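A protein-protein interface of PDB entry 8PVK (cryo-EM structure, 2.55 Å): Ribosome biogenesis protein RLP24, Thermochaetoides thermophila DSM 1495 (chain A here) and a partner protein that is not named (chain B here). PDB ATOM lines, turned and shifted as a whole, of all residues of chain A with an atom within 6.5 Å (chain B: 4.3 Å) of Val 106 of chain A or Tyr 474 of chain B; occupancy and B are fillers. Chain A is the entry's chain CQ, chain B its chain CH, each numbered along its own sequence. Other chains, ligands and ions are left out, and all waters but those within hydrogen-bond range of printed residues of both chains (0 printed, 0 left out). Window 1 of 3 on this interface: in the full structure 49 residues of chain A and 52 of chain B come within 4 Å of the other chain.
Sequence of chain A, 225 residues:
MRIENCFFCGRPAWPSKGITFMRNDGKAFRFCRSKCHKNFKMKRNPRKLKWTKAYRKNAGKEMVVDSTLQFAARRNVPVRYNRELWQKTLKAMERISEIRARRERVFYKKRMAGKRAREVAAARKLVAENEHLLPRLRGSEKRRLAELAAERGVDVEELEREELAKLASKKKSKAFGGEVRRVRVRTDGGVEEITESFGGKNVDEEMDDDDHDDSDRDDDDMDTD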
ATOM      1  N   ILE A  99      14.653  -9.816  37.471  1.00  0.00           N
ATOM      2  CA  ILE A  99      15.658 -10.783  37.028  1.00  0.00           C
ATOM      3  C   ILE A  99      15.079 -11.724  35.978  1.00  0.00           C
ATOM      4  O   ILE A  99      15.728 -12.024  34.964  1.00  0.00           O
ATOM      5  CB  ILE A  99      16.218 -11.553  38.239  1.00  0.00           C
ATOM      6  CG1 ILE A  99      16.996 -10.610  39.157  1.00  0.00           C
ATOM      7  CG2 ILE A  99      17.113 -12.695  37.797  1.00  0.00           C
ATOM      8  CD1 ILE A  99      17.367 -11.226  40.483  1.00  0.00           C
ATOM      9  N   ALA A 101      12.553 -11.149  33.914  1.00  0.00           N
ATOM     10  CA  ALA A 101      12.343 -10.440  32.654  1.00  0.00           C
ATOM     11  C   ALA A 101      13.639 -10.305  31.860  1.00  0.00           C
ATOM     12  O   ALA A 101      13.662 -10.542  30.641  1.00  0.00           O
ATOM     13  CB  ALA A 101      11.732  -9.066  32.922  1.00  0.00           C
ATOM     14  N   ARG A 102      14.739  -9.951  32.533  1.00  0.00           N
ATOM     15  CA  ARG A 102      15.978  -9.750  31.780  1.00  0.00           C
ATOM     16  C   ARG A 102      16.584 -11.081  31.315  1.00  0.00           C
ATOM     17  O   ARG A 102      17.122 -11.166  30.194  1.00  0.00           O
ATOM     18  CB  ARG A 102      16.920  -8.875  32.615  1.00  0.00           C
ATOM     19  CG  ARG A 102      17.448  -9.435  33.917  1.00  0.00           C
ATOM     20  CD  ARG A 102      18.300  -8.362  34.600  1.00  0.00           C
ATOM     21  NE  ARG A 102      19.532  -7.981  33.918  1.00  0.00           N
ATOM     22  CZ  ARG A 102      20.684  -8.622  34.042  1.00  0.00           C
ATOM     23  NH1 ARG A 102      20.795  -9.697  34.801  1.00  0.00           N
ATOM     24  NH2 ARG A 102      21.759  -8.149  33.419  1.00  0.00           N
ATOM     25  N   ARG A 103      16.418 -12.151  32.103  1.00  0.00           N
ATOM     26  CA  ARG A 103      16.804 -13.479  31.628  1.00  0.00           C
ATOM     27  C   ARG A 103      15.944 -13.946  30.457  1.00  0.00           C
ATOM     28  O   ARG A 103      16.452 -14.617  29.549  1.00  0.00           O
ATOM     29  CB  ARG A 103      16.729 -14.499  32.765  1.00  0.00           C
ATOM     30  CG  ARG A 103      17.774 -14.304  33.842  1.00  0.00           C
ATOM     31  CD  ARG A 103      17.813 -15.472  34.812  1.00  0.00           C
ATOM     32  NE  ARG A 103      18.873 -15.314  35.801  1.00  0.00           N
ATOM     33  CZ  ARG A 103      19.113 -16.166  36.787  1.00  0.00           C
ATOM     34  NH1 ARG A 103      18.384 -17.257  36.953  1.00  0.00           N
ATOM     35  NH2 ARG A 103      20.110 -15.916  37.631  1.00  0.00           N
ATOM     36  N   GLU A 104      14.649 -13.610  30.458  1.00  0.00           N
ATOM     37  CA  GLU A 104      13.782 -13.966  29.337  1.00  0.00           C
ATOM     38  C   GLU A 104      14.205 -13.250  28.061  1.00  0.00           C
ATOM     39  O   GLU A 104      14.138 -13.824  26.966  1.00  0.00           O
ATOM     40  CB  GLU A 104      12.328 -13.643  29.679  1.00  0.00           C
ATOM     41  CG  GLU A 104      11.301 -14.430  28.877  1.00  0.00           C
ATOM     42  CD  GLU A 104      10.957 -13.765  27.557  1.00  0.00           C
ATOM     43  OE1 GLU A 104      10.875 -12.520  27.525  1.00  0.00           O
ATOM     44  OE2 GLU A 104      10.772 -14.485  26.554  1.00  0.00           O
ATOM     45  N   ARG A 105      14.626 -11.987  28.184  1.00  0.00           N
ATOM     46  CA  ARG A 105      15.147 -11.272  27.018  1.00  0.00           C
ATOM     47  C   ARG A 105      16.404 -11.943  26.469  1.00  0.00           C
ATOM     48  O   ARG A 105      16.567 -12.076  25.245  1.00  0.00           O
ATOM     49  CB  ARG A 105      15.428  -9.812  27.375  1.00  0.00           C
ATOM     50  CG  ARG A 105      16.135  -9.040  26.274  1.00  0.00           C
ATOM     51  CD  ARG A 105      16.119  -7.547  26.531  1.00  0.00           C
ATOM     52  NE  ARG A 105      14.928  -6.918  25.975  1.00  0.00           N
ATOM     53  CZ  ARG A 105      14.885  -6.307  24.798  1.00  0.00           C
ATOM     54  NH1 ARG A 105      15.952  -6.230  24.020  1.00  0.00           N
ATOM     55  NH2 ARG A 105      13.743  -5.762  24.392  1.00  0.00           N
ATOM     56  N   VAL A 106      17.299 -12.386  27.363  1.00  0.00           N
ATOM     57  CA  VAL A 106      18.490 -13.115  26.916  1.00  0.00           C
ATOM     58  C   VAL A 106      18.104 -14.415  26.205  1.00  0.00           C
ATOM     59  O   VAL A 106      18.687 -14.774  25.169  1.00  0.00           O
ATOM     60  CB  VAL A 106      19.433 -13.370  28.108  1.00  0.00           C
ATOM     61  CG1 VAL A 106      20.605 -14.248  27.701  1.00  0.00           C
ATOM     62  CG2 VAL A 106      19.936 -12.052  28.654  1.00  0.00           C
ATOM     63  N   PHE A 107      17.103 -15.123  26.740  1.00  0.00           N
ATOM     64  CA  PHE A 107      16.614 -16.356  26.119  1.00  0.00           C
ATOM     65  C   PHE A 107      16.066 -16.102  24.717  1.00  0.00           C
ATOM     66  O   PHE A 107      16.334 -16.874  23.783  1.00  0.00           O
ATOM     67  CB  PHE A 107      15.544 -16.983  27.018  1.00  0.00           C
ATOM     68  CG  PHE A 107      14.984 -18.284  26.506  1.00  0.00           C
ATOM     69  CD1 PHE A 107      15.625 -19.482  26.772  1.00  0.00           C
ATOM     70  CD2 PHE A 107      13.789 -18.313  25.800  1.00  0.00           C
ATOM     71  CE1 PHE A 107      15.106 -20.681  26.316  1.00  0.00           C
ATOM     72  CE2 PHE A 107      13.266 -19.507  25.340  1.00  0.00           C
ATOM     73  CZ  PHE A 107      13.924 -20.692  25.600  1.00  0.00           C
ATOM     74  N   TYR A 108      15.305 -15.018  24.547  1.00  0.00           N
ATOM     75  CA  TYR A 108      14.750 -14.704  23.231  1.00  0.00           C
ATOM     76  C   TYR A 108      15.844 -14.337  22.234  1.00  0.00           C
ATOM     77  O   TYR A 108      15.762 -14.701  21.053  1.00  0.00           O
ATOM     78  CB  TYR A 108      13.727 -13.576  23.345  1.00  0.00           C
ATOM     79  CG  TYR A 108      12.937 -13.353  22.075  1.00  0.00           C
ATOM     80  CD1 TYR A 108      11.909 -14.212  21.715  1.00  0.00           C
ATOM     81  CD2 TYR A 108      13.220 -12.285  21.236  1.00  0.00           C
ATOM     82  CE1 TYR A 108      11.184 -14.014  20.556  1.00  0.00           C
ATOM     83  CE2 TYR A 108      12.501 -12.077  20.074  1.00  0.00           C
ATOM     84  CZ  TYR A 108      11.485 -12.945  19.739  1.00  0.00           C
ATOM     85  OH  TYR A 108      10.767 -12.743  18.584  1.00  0.00           O
ATOM     86  N   LYS A 109      16.875 -13.613  22.685  1.00  0.00           N
ATOM     87  CA  LYS A 109      17.986 -13.292  21.789  1.00  0.00           C
ATOM     88  C   LYS A 109      18.742 -14.550  21.362  1.00  0.00           C
ATOM     89  O   LYS A 109      19.152 -14.678  20.195  1.00  0.00           O
ATOM     90  CB  LYS A 109      18.930 -12.296  22.459  1.00  0.00           C
ATOM     91  CG  LYS A 109      18.755 -10.870  21.968  1.00  0.00           C
ATOM     92  CD  LYS A 109      19.472  -9.881  22.870  1.00  0.00           C
ATOM     93  CE  LYS A 109      19.096  -8.450  22.523  1.00  0.00           C
ATOM     94  NZ  LYS A 109      19.139  -7.560  23.716  1.00  0.00           N
ATOM     95  N   LYS A 110      18.937 -15.489  22.294  1.00  0.00           N
ATOM     96  CA  LYS A 110      19.555 -16.762  21.928  1.00  0.00           C
ATOM     97  C   LYS A 110      18.681 -17.556  20.964  1.00  0.00           C
ATOM     98  O   LYS A 110      19.205 -18.321  20.146  1.00  0.00           O
ATOM     99  CB  LYS A 110      19.859 -17.593  23.174  1.00  0.00           C
ATOM    100  CG  LYS A 110      20.934 -16.995  24.063  1.00  0.00           C
ATOM    101  CD  LYS A 110      21.228 -17.894  25.250  1.00  0.00           C
ATOM    102  CE  LYS A 110      22.246 -17.258  26.180  1.00  0.00           C
ATOM    103  NZ  LYS A 110      23.589 -17.159  25.543  1.00  0.00           N
ATOM    104  N   ARG A 111      17.358 -17.401  21.050  1.00  0.00           N
ATOM    105  CA  ARG A 111      16.489 -18.024  20.054  1.00  0.00           C
ATOM    106  C   ARG A 111      16.634 -17.364  18.684  1.00  0.00           C
ATOM    107  O   ARG A 111      16.581 -18.045  17.655  1.00  0.00           O
ATOM    108  CB  ARG A 111      15.032 -17.978  20.512  1.00  0.00           C
ATOM    109  CG  ARG A 111      14.709 -18.912  21.664  1.00  0.00           C
ATOM    110  CD  ARG A 111      13.357 -19.583  21.474  1.00  0.00           C
ATOM    111  NE  ARG A 111      12.259 -18.624  21.426  1.00  0.00           N
ATOM    112  CZ  ARG A 111      11.404 -18.515  20.418  1.00  0.00           C
ATOM    113  NH1 ARG A 111      11.490 -19.290  19.352  1.00  0.00           N
ATOM    114  NH2 ARG A 111      10.436 -17.605  20.486  1.00  0.00           N
ATOM    115  N   GLU B 465      23.253 -14.412  40.234  1.00  0.00           N
ATOM    116  CA  GLU B 465      23.161 -13.237  39.365  1.00  0.00           C
ATOM    117  C   GLU B 465      24.512 -12.547  39.174  1.00  0.00           C
ATOM    118  O   GLU B 465      24.916 -12.279  38.036  1.00  0.00           O
ATOM    119  CB  GLU B 465      22.120 -12.254  39.906  1.00  0.00           C
ATOM    120  CG  GLU B 465      21.833 -11.075  38.983  1.00  0.00           C
ATOM    121  CD  GLU B 465      20.893 -11.407  37.835  1.00  0.00           C
ATOM    122  OE1 GLU B 465      20.433 -12.564  37.737  1.00  0.00           O
ATOM    123  OE2 GLU B 465      20.607 -10.500  37.026  1.00  0.00           O
ATOM    124  N   LEU B 468      26.579 -14.866  36.939  1.00  0.00           N
ATOM    125  CA  LEU B 468      26.260 -14.724  35.524  1.00  0.00           C
ATOM    126  C   LEU B 468      26.766 -13.398  34.965  1.00  0.00           C
ATOM    127  O   LEU B 468      27.128 -13.324  33.787  1.00  0.00           O
ATOM    128  CB  LEU B 468      24.751 -14.865  35.319  1.00  0.00           C
ATOM    129  CG  LEU B 468      24.161 -16.264  35.506  1.00  0.00           C
ATOM    130  CD1 LEU B 468      22.664 -16.263  35.246  1.00  0.00           C
ATOM    131  CD2 LEU B 468      24.853 -17.284  34.625  1.00  0.00           C
ATOM    132  N   GLY B 472      29.559 -13.082  32.199  1.00  0.00           N
ATOM    133  CA  GLY B 472      28.985 -12.309  31.106  1.00  0.00           C
ATOM    134  C   GLY B 472      27.799 -12.931  30.403  1.00  0.00           C
ATOM    135  O   GLY B 472      27.757 -12.952  29.167  1.00  0.00           O
ATOM    136  N   PHE B 473      26.835 -13.451  31.163  1.00  0.00           N
ATOM    137  CA  PHE B 473      25.647 -14.055  30.575  1.00  0.00           C
ATOM    138  C   PHE B 473      24.731 -13.017  29.934  1.00  0.00           C
ATOM    139  O   PHE B 473      23.928 -13.368  29.063  1.00  0.00           O
ATOM    140  CB  PHE B 473      24.912 -14.846  31.663  1.00  0.00           C
ATOM    141  CG  PHE B 473      23.679 -15.560  31.190  1.00  0.00           C
ATOM    142  CD1 PHE B 473      23.780 -16.775  30.534  1.00  0.00           C
ATOM    143  CD2 PHE B 473      22.419 -15.038  31.436  1.00  0.00           C
ATOM    144  CE1 PHE B 473      22.650 -17.445  30.108  1.00  0.00           C
ATOM    145  CE2 PHE B 473      21.284 -15.702  31.014  1.00  0.00           C
ATOM    146  CZ  PHE B 473      21.400 -16.908  30.349  1.00  0.00           C
ATOM    147  N   TYR B 474      24.857 -11.747  30.318  1.00  0.00           N
ATOM    148  CA  TYR B 474      23.946 -10.698  29.882  1.00  0.00           C
ATOM    149  C   TYR B 474      24.601  -9.664  28.971  1.00  0.00           C
ATOM    150  O   TYR B 474      24.025  -8.591  28.765  1.00  0.00           O
ATOM    151  CB  TYR B 474      23.344  -9.995  31.099  1.00  0.00           C
ATOM    152  CG  TYR B 474      22.660 -10.928  32.067  1.00  0.00           C
ATOM    153  CD1 TYR B 474      21.355 -11.345  31.852  1.00  0.00           C
ATOM    154  CD2 TYR B 474      23.317 -11.389  33.200  1.00  0.00           C
ATOM    155  CE1 TYR B 474      20.721 -12.200  32.732  1.00  0.00           C
ATOM    156  CE2 TYR B 474      22.694 -12.243  34.088  1.00  0.00           C
ATOM    157  CZ  TYR B 474      21.397 -12.646  33.850  1.00  0.00           C
ATOM    158  OH  TYR B 474      20.780 -13.494  34.739  1.00  0.00           O
ATOM    159  N   ASP B 475      25.783  -9.947  28.428  1.00  0.00           N
ATOM    160  CA  ASP B 475      26.450  -8.960  27.593  1.00  0.00           C
ATOM    161  C   ASP B 475      25.794  -8.870  26.216  1.00  0.00           C
ATOM    162  O   ASP B 475      25.121  -9.795  25.752  1.00  0.00           O
ATOM    163  CB  ASP B 475      27.943  -9.278  27.452  1.00  0.00           C
ATOM    164  CG  ASP B 475      28.213 -10.723  27.060  1.00  0.00           C
ATOM    165  OD1 ASP B 475      27.263 -11.463  26.727  1.00  0.00           O
ATOM    166  OD2 ASP B 475      29.396 -11.122  27.082  1.00  0.00           O
ATOM    167  N   GLU B 476      25.997  -7.730  25.562  1.00  0.00           N
ATOM    168  CA  GLU B 476      25.443  -7.471  24.243  1.00  0.00           C
ATOM    169  C   GLU B 476      26.564  -7.192  23.252  1.00  0.00           C
ATOM    170  O   GLU B 476      27.591  -6.600  23.599  1.00  0.00           O
ATOM    171  CB  GLU B 476      24.466  -6.289  24.270  1.00  0.00           C
ATOM    172  CG  GLU B 476      23.307  -6.461  25.237  1.00  0.00           C
ATOM    173  CD  GLU B 476      22.311  -5.319  25.164  1.00  0.00           C
ATOM    174  OE1 GLU B 476      22.508  -4.409  24.331  1.00  0.00           O
ATOM    175  OE2 GLU B 476      21.332  -5.331  25.939  1.00  0.00           O
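The side-chain carboxylate (OE1) of Glu 465 of chain B is in salt-bridge range of the guanidinium group (NH2) of Arg 103 of chain A (3.4 Å). OH of Tyr 474 of chain B sits at hydrogen-bond distance from NE of Arg 103 of chain A. NZ of Lys 109 of chain A lies within salt-bridge range of OE2 of Glu 476 of chain B (3.8 Å). The guanidinium group (NH1) of Arg 102 of chain A lies close to the side-chain carboxylate (OE2) of Glu 465 of chain B, 2.4 Å away.
The side-chain carboxylate (OE1) of Glu 465 of chain B sits at hydrogen-bond distance from the side-chain hydroxyl (OH) of Tyr 474 of chain B, at 3.2 Å. The backbone carbonyl oxygen (O) of Leu 468 of chain B is in hydrogen-bond range of the backbone NH (N) of Phe 473 of chain B (2.6 Å).
CG2 of Ile 99 of chain A touches OE1 of Glu 465 of chain B (3.3 Å). Arg 102 of chain A touches Tyr 474 of chain B (NH1 to CZ, 3.2 Å). Arg 103 of chain A touches Leu 468 of chain B. Phe 473 of chain B touches Val 106 of chain A. Val 106 of chain A touches Tyr 474 of chain B (CG2 to CD1, 3.6 Å). Phe 473 of chain B touches Lys 110 of chain A.
Of chain B, only Phe 473 (3.7 Å) and Tyr 474 (3.6 Å) come within 4 Å of Val 106 of chain A. Tyr 474 of chain B touches just these residues of chain A: Arg 102, Arg 103 and Val 106. Of the printed residues of chain B, Lys 109 of chain A touches Glu 476 (3.8 Å). Of the printed residues of chain A, Glu 465 of chain B touches Ile 99 (3.3 Å), Arg 102 (2.4 Å) and Arg 103 (3.4 Å). Of the printed residues of chain B, Ile 99 of chain A touches Glu 465. Arg 105 of chain A touches none of the printed residues of chain B. The nearest residue of chain A that does not touch Tyr 474 of chain B is Ile 99 of chain A (4.8 Å). The nearest printed residue of chain B that does not touch Lys 109 of chain A is Asp 475 of chain B (6.3 Å).
Hydrophobic or aromatic side chains of chain B that line the printed part of chain A: Leu 468, Phe 473 and Tyr 474. Of the 12 printed residues of chain A, 6 touch a printed residue of chain B. Hydrophobic or aromatic side chains of chain A that line the printed part of chain B: Ile 99 and Val 106. Among the printed residues, 10 pairs touch across the chains. Among the printed residues, Asp or Glu carboxylates within 4 Å of a Lys or Arg side-chain nitrogen of the other chain: Arg 102 of chain A with Glu 465 of chain B, Arg 103 of chain A with Glu 465 of chain B and Lys 109 of chain A with Glu 476 of chain B.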
